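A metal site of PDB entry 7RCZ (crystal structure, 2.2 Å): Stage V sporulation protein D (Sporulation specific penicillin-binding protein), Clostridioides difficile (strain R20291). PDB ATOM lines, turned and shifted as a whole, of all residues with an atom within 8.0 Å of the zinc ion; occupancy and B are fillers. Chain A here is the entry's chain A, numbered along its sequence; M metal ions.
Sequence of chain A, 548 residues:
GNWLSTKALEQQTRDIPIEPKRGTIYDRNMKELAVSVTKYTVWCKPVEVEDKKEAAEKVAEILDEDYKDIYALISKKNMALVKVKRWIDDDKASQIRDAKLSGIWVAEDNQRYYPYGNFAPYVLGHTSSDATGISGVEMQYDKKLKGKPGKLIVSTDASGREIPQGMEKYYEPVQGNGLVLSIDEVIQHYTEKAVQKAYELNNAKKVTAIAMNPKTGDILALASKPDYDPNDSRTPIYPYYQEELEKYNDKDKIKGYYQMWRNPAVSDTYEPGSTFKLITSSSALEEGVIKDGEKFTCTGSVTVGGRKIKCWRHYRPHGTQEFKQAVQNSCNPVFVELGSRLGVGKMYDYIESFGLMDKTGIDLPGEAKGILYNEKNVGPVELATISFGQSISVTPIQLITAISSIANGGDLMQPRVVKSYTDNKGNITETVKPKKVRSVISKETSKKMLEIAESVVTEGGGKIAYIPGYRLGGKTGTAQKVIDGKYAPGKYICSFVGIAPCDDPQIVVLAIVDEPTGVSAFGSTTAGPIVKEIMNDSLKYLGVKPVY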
ATOM      1  N   PHE A 296       9.079 -36.459 -19.222  1.00  0.00           N
ATOM      2  CA  PHE A 296       7.907 -35.557 -19.148  1.00  0.00           C
ATOM      3  C   PHE A 296       7.723 -34.892 -20.510  1.00  0.00           C
ATOM      4  O   PHE A 296       8.667 -34.248 -21.037  1.00  0.00           O
ATOM      5  CB  PHE A 296       8.077 -34.458 -18.092  1.00  0.00           C
ATOM      6  CG  PHE A 296       8.507 -34.939 -16.736  1.00  0.00           C
ATOM      7  CD1 PHE A 296       9.835 -35.270 -16.486  1.00  0.00           C
ATOM      8  CD2 PHE A 296       7.596 -35.029 -15.691  1.00  0.00           C
ATOM      9  CE1 PHE A 296      10.219 -35.716 -15.237  1.00  0.00           C
ATOM     10  CE2 PHE A 296       7.996 -35.451 -14.439  1.00  0.00           C
ATOM     11  CZ  PHE A 296       9.300 -35.807 -14.214  1.00  0.00           C
ATOM     12  N   THR A 297       6.515 -34.997 -21.041  1.00  0.00           N
ATOM     13  CA  THR A 297       6.160 -34.513 -22.404  1.00  0.00           C
ATOM     14  C   THR A 297       5.549 -33.123 -22.308  1.00  0.00           C
ATOM     15  O   THR A 297       4.514 -32.961 -21.634  1.00  0.00           O
ATOM     16  CB  THR A 297       5.176 -35.459 -23.103  1.00  0.00           C
ATOM     17  OG1 THR A 297       5.874 -36.697 -23.174  1.00  0.00           O
ATOM     18  CG2 THR A 297       4.748 -34.963 -24.466  1.00  0.00           C
ATOM     19  N   CYS A 298       6.173 -32.179 -22.986  1.00  0.00           N
ATOM     20  CA  CYS A 298       5.615 -30.845 -23.270  1.00  0.00           C
ATOM     21  C   CYS A 298       4.863 -30.896 -24.612  1.00  0.00           C
ATOM     22  O   CYS A 298       5.520 -31.171 -25.624  1.00  0.00           O
ATOM     23  CB  CYS A 298       6.717 -29.795 -23.317  1.00  0.00           C
ATOM     24  SG  CYS A 298       6.050 -28.165 -23.691  1.00  0.00           S
ATOM     25  N   THR A 299       3.554 -30.603 -24.598  1.00  0.00           N
ATOM     26  CA  THR A 299       2.699 -30.334 -25.792  1.00  0.00           C
ATOM     27  C   THR A 299       2.419 -28.839 -25.882  1.00  0.00           C
ATOM     28  O   THR A 299       1.614 -28.442 -26.710  1.00  0.00           O
ATOM     29  CB  THR A 299       1.361 -31.073 -25.737  1.00  0.00           C
ATOM     30  OG1 THR A 299       0.531 -30.446 -24.747  1.00  0.00           O
ATOM     31  CG2 THR A 299       1.520 -32.544 -25.407  1.00  0.00           C
ATOM     32  N   GLY A 300       3.065 -28.039 -25.027  1.00  0.00           N
ATOM     33  CA  GLY A 300       2.958 -26.566 -25.055  1.00  0.00           C
ATOM     34  C   GLY A 300       1.948 -26.047 -24.049  1.00  0.00           C
ATOM     35  O   GLY A 300       1.940 -24.824 -23.793  1.00  0.00           O
ATOM     36  N   SER A 301       1.106 -26.916 -23.494  1.00  0.00           N
ATOM     37  CA  SER A 301       0.142 -26.492 -22.437  1.00  0.00           C
ATOM     38  C   SER A 301      -0.354 -27.685 -21.605  1.00  0.00           C
ATOM     39  O   SER A 301      -0.154 -28.855 -22.016  1.00  0.00           O
ATOM     40  CB  SER A 301      -1.020 -25.714 -23.032  1.00  0.00           C
ATOM     41  OG  SER A 301      -1.874 -26.575 -23.779  1.00  0.00           O
ATOM     42  N   LYS A 310       0.164 -22.283 -20.285  1.00  0.00           N
ATOM     43  CA  LYS A 310       1.034 -22.480 -21.488  1.00  0.00           C
ATOM     44  C   LYS A 310       2.503 -22.549 -21.052  1.00  0.00           C
ATOM     45  O   LYS A 310       2.905 -21.788 -20.157  1.00  0.00           O
ATOM     46  CB  LYS A 310       0.883 -21.327 -22.482  1.00  0.00           C
ATOM     47  CG  LYS A 310      -0.497 -21.137 -23.116  1.00  0.00           C
ATOM     48  CD  LYS A 310      -0.698 -19.725 -23.692  1.00  0.00           C
ATOM     49  CE  LYS A 310      -2.044 -19.510 -24.359  1.00  0.00           C
ATOM     50  NZ  LYS A 310      -1.929 -19.455 -25.843  1.00  0.00           N
ATOM     51  N   CYS A 311       3.276 -23.412 -21.705  1.00  0.00           N
ATOM     52  CA  CYS A 311       4.740 -23.331 -21.789  1.00  0.00           C
ATOM     53  C   CYS A 311       5.075 -21.986 -22.445  1.00  0.00           C
ATOM     54  O   CYS A 311       4.253 -21.498 -23.253  1.00  0.00           O
ATOM     55  CB  CYS A 311       5.283 -24.531 -22.550  1.00  0.00           C
ATOM     56  SG  CYS A 311       7.079 -24.742 -22.474  1.00  0.00           S
ATOM     57  N   TRP A 312       6.201 -21.357 -22.082  1.00  0.00           N
ATOM     58  CA  TRP A 312       6.690 -20.123 -22.748  1.00  0.00           C
ATOM     59  C   TRP A 312       6.900 -20.402 -24.243  1.00  0.00           C
ATOM     60  O   TRP A 312       6.722 -19.467 -25.037  1.00  0.00           O
ATOM     61  CB  TRP A 312       7.957 -19.592 -22.049  1.00  0.00           C
ATOM     62  CG  TRP A 312       9.190 -20.370 -22.391  1.00  0.00           C
ATOM     63  CD1 TRP A 312       9.697 -21.434 -21.709  1.00  0.00           C
ATOM     64  CD2 TRP A 312      10.048 -20.159 -23.533  1.00  0.00           C
ATOM     65  NE1 TRP A 312      10.814 -21.909 -22.349  1.00  0.00           N
ATOM     66  CE2 TRP A 312      11.058 -21.141 -23.460  1.00  0.00           C
ATOM     67  CE3 TRP A 312      10.069 -19.229 -24.579  1.00  0.00           C
ATOM     68  CZ2 TRP A 312      12.074 -21.219 -24.411  1.00  0.00           C
ATOM     69  CZ3 TRP A 312      11.085 -19.311 -25.506  1.00  0.00           C
ATOM     70  CH2 TRP A 312      12.076 -20.291 -25.421  1.00  0.00           C
ATOM     71  N   ARG A 313       7.236 -21.654 -24.599  1.00  0.00           N
ATOM     72  CA  ARG A 313       7.540 -22.088 -25.987  1.00  0.00           C
ATOM     73  C   ARG A 313       6.413 -23.007 -26.496  1.00  0.00           C
ATOM     74  O   ARG A 313       6.744 -24.007 -27.155  1.00  0.00           O
ATOM     75  CB  ARG A 313       8.912 -22.775 -26.035  1.00  0.00           C
ATOM     76  CG  ARG A 313       9.831 -22.233 -27.123  1.00  0.00           C
ATOM     77  CD  ARG A 313      11.118 -23.018 -27.283  1.00  0.00           C
ATOM     78  NE  ARG A 313      10.792 -24.360 -27.742  1.00  0.00           N
ATOM     79  CZ  ARG A 313      11.634 -25.379 -27.866  1.00  0.00           C
ATOM     80  NH1 ARG A 313      12.920 -25.245 -27.597  1.00  0.00           N
ATOM     81  NH2 ARG A 313      11.163 -26.528 -28.291  1.00  0.00           N
ATOM     82  N   HIS A 314       5.148 -22.643 -26.218  1.00  0.00           N
ATOM     83  CA  HIS A 314       3.919 -23.410 -26.575  1.00  0.00           C
ATOM     84  C   HIS A 314       3.683 -23.454 -28.087  1.00  0.00           C
ATOM     85  O   HIS A 314       2.896 -24.297 -28.535  1.00  0.00           O
ATOM     86  CB  HIS A 314       2.665 -22.796 -25.908  1.00  0.00           C
ATOM     87  CG  HIS A 314       2.204 -21.519 -26.522  1.00  0.00           C
ATOM     88  ND1 HIS A 314       1.097 -21.463 -27.352  1.00  0.00           N
ATOM     89  CD2 HIS A 314       2.699 -20.264 -26.441  1.00  0.00           C
ATOM     90  CE1 HIS A 314       0.921 -20.216 -27.746  1.00  0.00           C
ATOM     91  NE2 HIS A 314       1.891 -19.456 -27.210  1.00  0.00           N
ATOM     92  N   ARG A 316       6.213 -23.917 -30.116  1.00  0.00           N
ATOM     93  CA  ARG A 316       7.191 -24.981 -30.461  1.00  0.00           C
ATOM     94  C   ARG A 316       7.440 -25.851 -29.230  1.00  0.00           C
ATOM     95  O   ARG A 316       8.468 -25.755 -28.556  1.00  0.00           O
ATOM     96  CB  ARG A 316       8.460 -24.353 -31.054  1.00  0.00           C
ATOM     97  CG  ARG A 316       9.216 -25.285 -31.988  1.00  0.00           C
ATOM     98  CD  ARG A 316       9.857 -24.560 -33.158  1.00  0.00           C
ATOM     99  NE  ARG A 316       8.984 -23.530 -33.724  1.00  0.00           N
ATOM    100  CZ  ARG A 316       7.964 -23.744 -34.552  1.00  0.00           C
ATOM    101  NH1 ARG A 316       7.254 -22.716 -34.976  1.00  0.00           N
ATOM    102  NH2 ARG A 316       7.656 -24.962 -34.958  1.00  0.00           N
ATOM    103  N   PRO A 317       6.505 -26.771 -28.925  1.00  0.00           N
ATOM    104  CA  PRO A 317       6.601 -27.610 -27.726  1.00  0.00           C
ATOM    105  C   PRO A 317       7.972 -28.289 -27.514  1.00  0.00           C
ATOM    106  O   PRO A 317       8.626 -28.682 -28.507  1.00  0.00           O
ATOM    107  CB  PRO A 317       5.538 -28.693 -27.986  1.00  0.00           C
ATOM    108  CG  PRO A 317       4.502 -28.004 -28.869  1.00  0.00           C
ATOM    109  CD  PRO A 317       5.302 -27.044 -29.723  1.00  0.00           C
ATOM    110  N   HIS A 318       8.369 -28.461 -26.247  1.00  0.00           N
ATOM    111  CA  HIS A 318       9.637 -29.126 -25.851  1.00  0.00           C
ATOM    112  C   HIS A 318       9.565 -30.635 -26.102  1.00  0.00           C
ATOM    113  O   HIS A 318      10.640 -31.257 -26.140  1.00  0.00           O
ATOM    114  CB  HIS A 318       9.974 -28.845 -24.394  1.00  0.00           C
ATOM    115  CG  HIS A 318      10.309 -27.414 -24.139  1.00  0.00           C
ATOM    116  ND1 HIS A 318       9.481 -26.591 -23.434  1.00  0.00           N
ATOM    117  CD2 HIS A 318      11.378 -26.667 -24.511  1.00  0.00           C
ATOM    118  CE1 HIS A 318      10.025 -25.388 -23.370  1.00  0.00           C
ATOM    119  NE2 HIS A 318      11.172 -25.400 -24.048  1.00  0.00           N
ATOM    120  N   GLY A 319       8.355 -31.205 -26.217  1.00  0.00           N
ATOM    121  CA  GLY A 319       8.179 -32.671 -26.371  1.00  0.00           C
ATOM    122  C   GLY A 319       8.706 -33.426 -25.161  1.00  0.00           C
ATOM    123  O   GLY A 319       8.532 -32.944 -24.032  1.00  0.00           O
ATOM    124  N   GLN A 321      11.109 -34.786 -22.362  1.00  0.00           N
ATOM    125  CA  GLN A 321      12.229 -34.202 -21.573  1.00  0.00           C
ATOM    126  C   GLN A 321      12.521 -35.087 -20.363  1.00  0.00           C
ATOM    127  O   GLN A 321      11.568 -35.440 -19.656  1.00  0.00           O
ATOM    128  CB  GLN A 321      11.902 -32.780 -21.085  1.00  0.00           C
ATOM    129  CG  GLN A 321      11.486 -31.809 -22.176  1.00  0.00           C
ATOM    130  CD  GLN A 321      10.780 -30.582 -21.620  1.00  0.00           C
ATOM    131  OE1 GLN A 321      11.400 -29.548 -21.395  1.00  0.00           O
ATOM    132  NE2 GLN A 321       9.470 -30.698 -21.418  1.00  0.00           N
ATOM    133  N   ALA A 326      13.965 -30.305 -18.478  1.00  0.00           N
ATOM    134  CA  ALA A 326      12.758 -29.499 -18.215  1.00  0.00           C
ATOM    135  C   ALA A 326      13.117 -28.233 -17.407  1.00  0.00           C
ATOM    136  O   ALA A 326      12.518 -27.170 -17.664  1.00  0.00           O
ATOM    137  CB  ALA A 326      11.696 -30.318 -17.526  1.00  0.00           C
ATOM    138  N   ASN A 329      14.943 -25.995 -19.779  1.00  0.00           N
ATOM    139  CA  ASN A 329      13.943 -25.484 -20.748  1.00  0.00           C
ATOM    140  C   ASN A 329      12.948 -24.543 -20.086  1.00  0.00           C
ATOM    141  O   ASN A 329      12.168 -23.890 -20.824  1.00  0.00           O
ATOM    142  CB  ASN A 329      13.182 -26.621 -21.425  1.00  0.00           C
ATOM    143  CG  ASN A 329      14.062 -27.428 -22.358  1.00  0.00           C
ATOM    144  OD1 ASN A 329      15.039 -26.897 -22.886  1.00  0.00           O
ATOM    145  ND2 ASN A 329      13.766 -28.702 -22.532  1.00  0.00           N
ATOM    146  N   SER A 330      12.939 -24.475 -18.757  1.00  0.00           N
ATOM    147  CA  SER A 330      11.947 -23.732 -17.942  1.00  0.00           C
ATOM    148  C   SER A 330      10.517 -24.085 -18.413  1.00  0.00           C
ATOM    149  O   SER A 330       9.686 -23.200 -18.593  1.00  0.00           O
ATOM    150  CB  SER A 330      12.228 -22.249 -18.022  1.00  0.00           C
ATOM    151  OG  SER A 330      11.666 -21.604 -16.893  1.00  0.00           O
ATOM    152  N   CYS A 331      10.265 -25.374 -18.608  1.00  0.00           N
ATOM    153  CA  CYS A 331       9.002 -25.900 -19.179  1.00  0.00           C
ATOM    154  C   CYS A 331       7.887 -25.893 -18.115  1.00  0.00           C
ATOM    155  O   CYS A 331       7.867 -26.800 -17.301  1.00  0.00           O
ATOM    156  CB  CYS A 331       9.251 -27.303 -19.699  1.00  0.00           C
ATOM    157  SG  CYS A 331       7.799 -27.961 -20.529  1.00  0.00           S
ATOM    158  N   ASN A 332       7.012 -24.895 -18.121  1.00  0.00           N
ATOM    159  CA  ASN A 332       5.941 -24.700 -17.103  1.00  0.00           C
ATOM    160  C   ASN A 332       5.109 -25.956 -16.878  1.00  0.00           C
ATOM    161  O   ASN A 332       4.926 -26.349 -15.729  1.00  0.00           O
ATOM    162  CB  ASN A 332       5.047 -23.503 -17.444  1.00  0.00           C
ATOM    163  CG  ASN A 332       5.742 -22.204 -17.168  1.00  0.00           C
ATOM    164  OD1 ASN A 332       6.840 -22.195 -16.606  1.00  0.00           O
ATOM    165  ND2 ASN A 332       5.120 -21.101 -17.556  1.00  0.00           N
ATOM    166  N   PRO A 333       4.560 -26.622 -17.929  1.00  0.00           N
ATOM    167  CA  PRO A 333       3.709 -27.800 -17.704  1.00  0.00           C
ATOM    168  C   PRO A 333       4.373 -28.845 -16.814  1.00  0.00           C
ATOM    169  O   PRO A 333       3.677 -29.395 -16.007  1.00  0.00           O
ATOM    170  CB  PRO A 333       3.460 -28.317 -19.117  1.00  0.00           C
ATOM    171  CG  PRO A 333       3.415 -27.029 -19.915  1.00  0.00           C
ATOM    172  CD  PRO A 333       4.578 -26.233 -19.350  1.00  0.00           C
ATOM    173  N   VAL A 334       5.677 -29.070 -16.943  1.00  0.00           N
ATOM    174  CA  VAL A 334       6.385 -30.092 -16.120  1.00  0.00           C
ATOM    175  C   VAL A 334       6.324 -29.667 -14.654  1.00  0.00           C
ATOM    176  O   VAL A 334       6.189 -30.545 -13.781  1.00  0.00           O
ATOM    177  CB  VAL A 334       7.836 -30.310 -16.591  1.00  0.00           C
ATOM    178  CG1 VAL A 334       8.597 -31.245 -15.665  1.00  0.00           C
ATOM    179  CG2 VAL A 334       7.912 -30.813 -18.041  1.00  0.00           C
HETATM  180 ZN    ZN M   1       7.610 -26.823 -22.541  1.00  0.00          ZN
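The backbone NH (N) of Cys 311 is in hydrogen-bond range of the backbone carbonyl oxygen (O) of Gly 300 (2.9 Å).
N of Arg 313 lies close to SG of Cys 311 (3.8 Å).
NE2 of Gln 321 sits close to SG of Cys 331, at 3.3 Å.
The backbone NH (N) of Cys 331 is in hydrogen-bond range of the backbone carbonyl oxygen (O) of Ala 326 (3.0 Å).
The side-chain sulfur (SG) of Cys 298 sits close to the backbone NH (N) of Gly 300 (3.3 Å).
N of Cys 298 lies within hydrogen-bond range of O of Gly 319, at 2.7 Å.
Four residues have an atom within 4 Å of the zinc ion: Cys 298, Cys 311, His 318 and Cys 331.
The nearest printed residue that does not touch the zinc ion is Pro 333 (4.4 Å).
ND1 of His 318 binds the zinc ion (2.1 Å).
The zinc ion is bound by SG of Cys 311 (2.1 Å).
The zinc ion is bound by SG of Cys 331.
The zinc ion is bound by SG of Cys 298.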
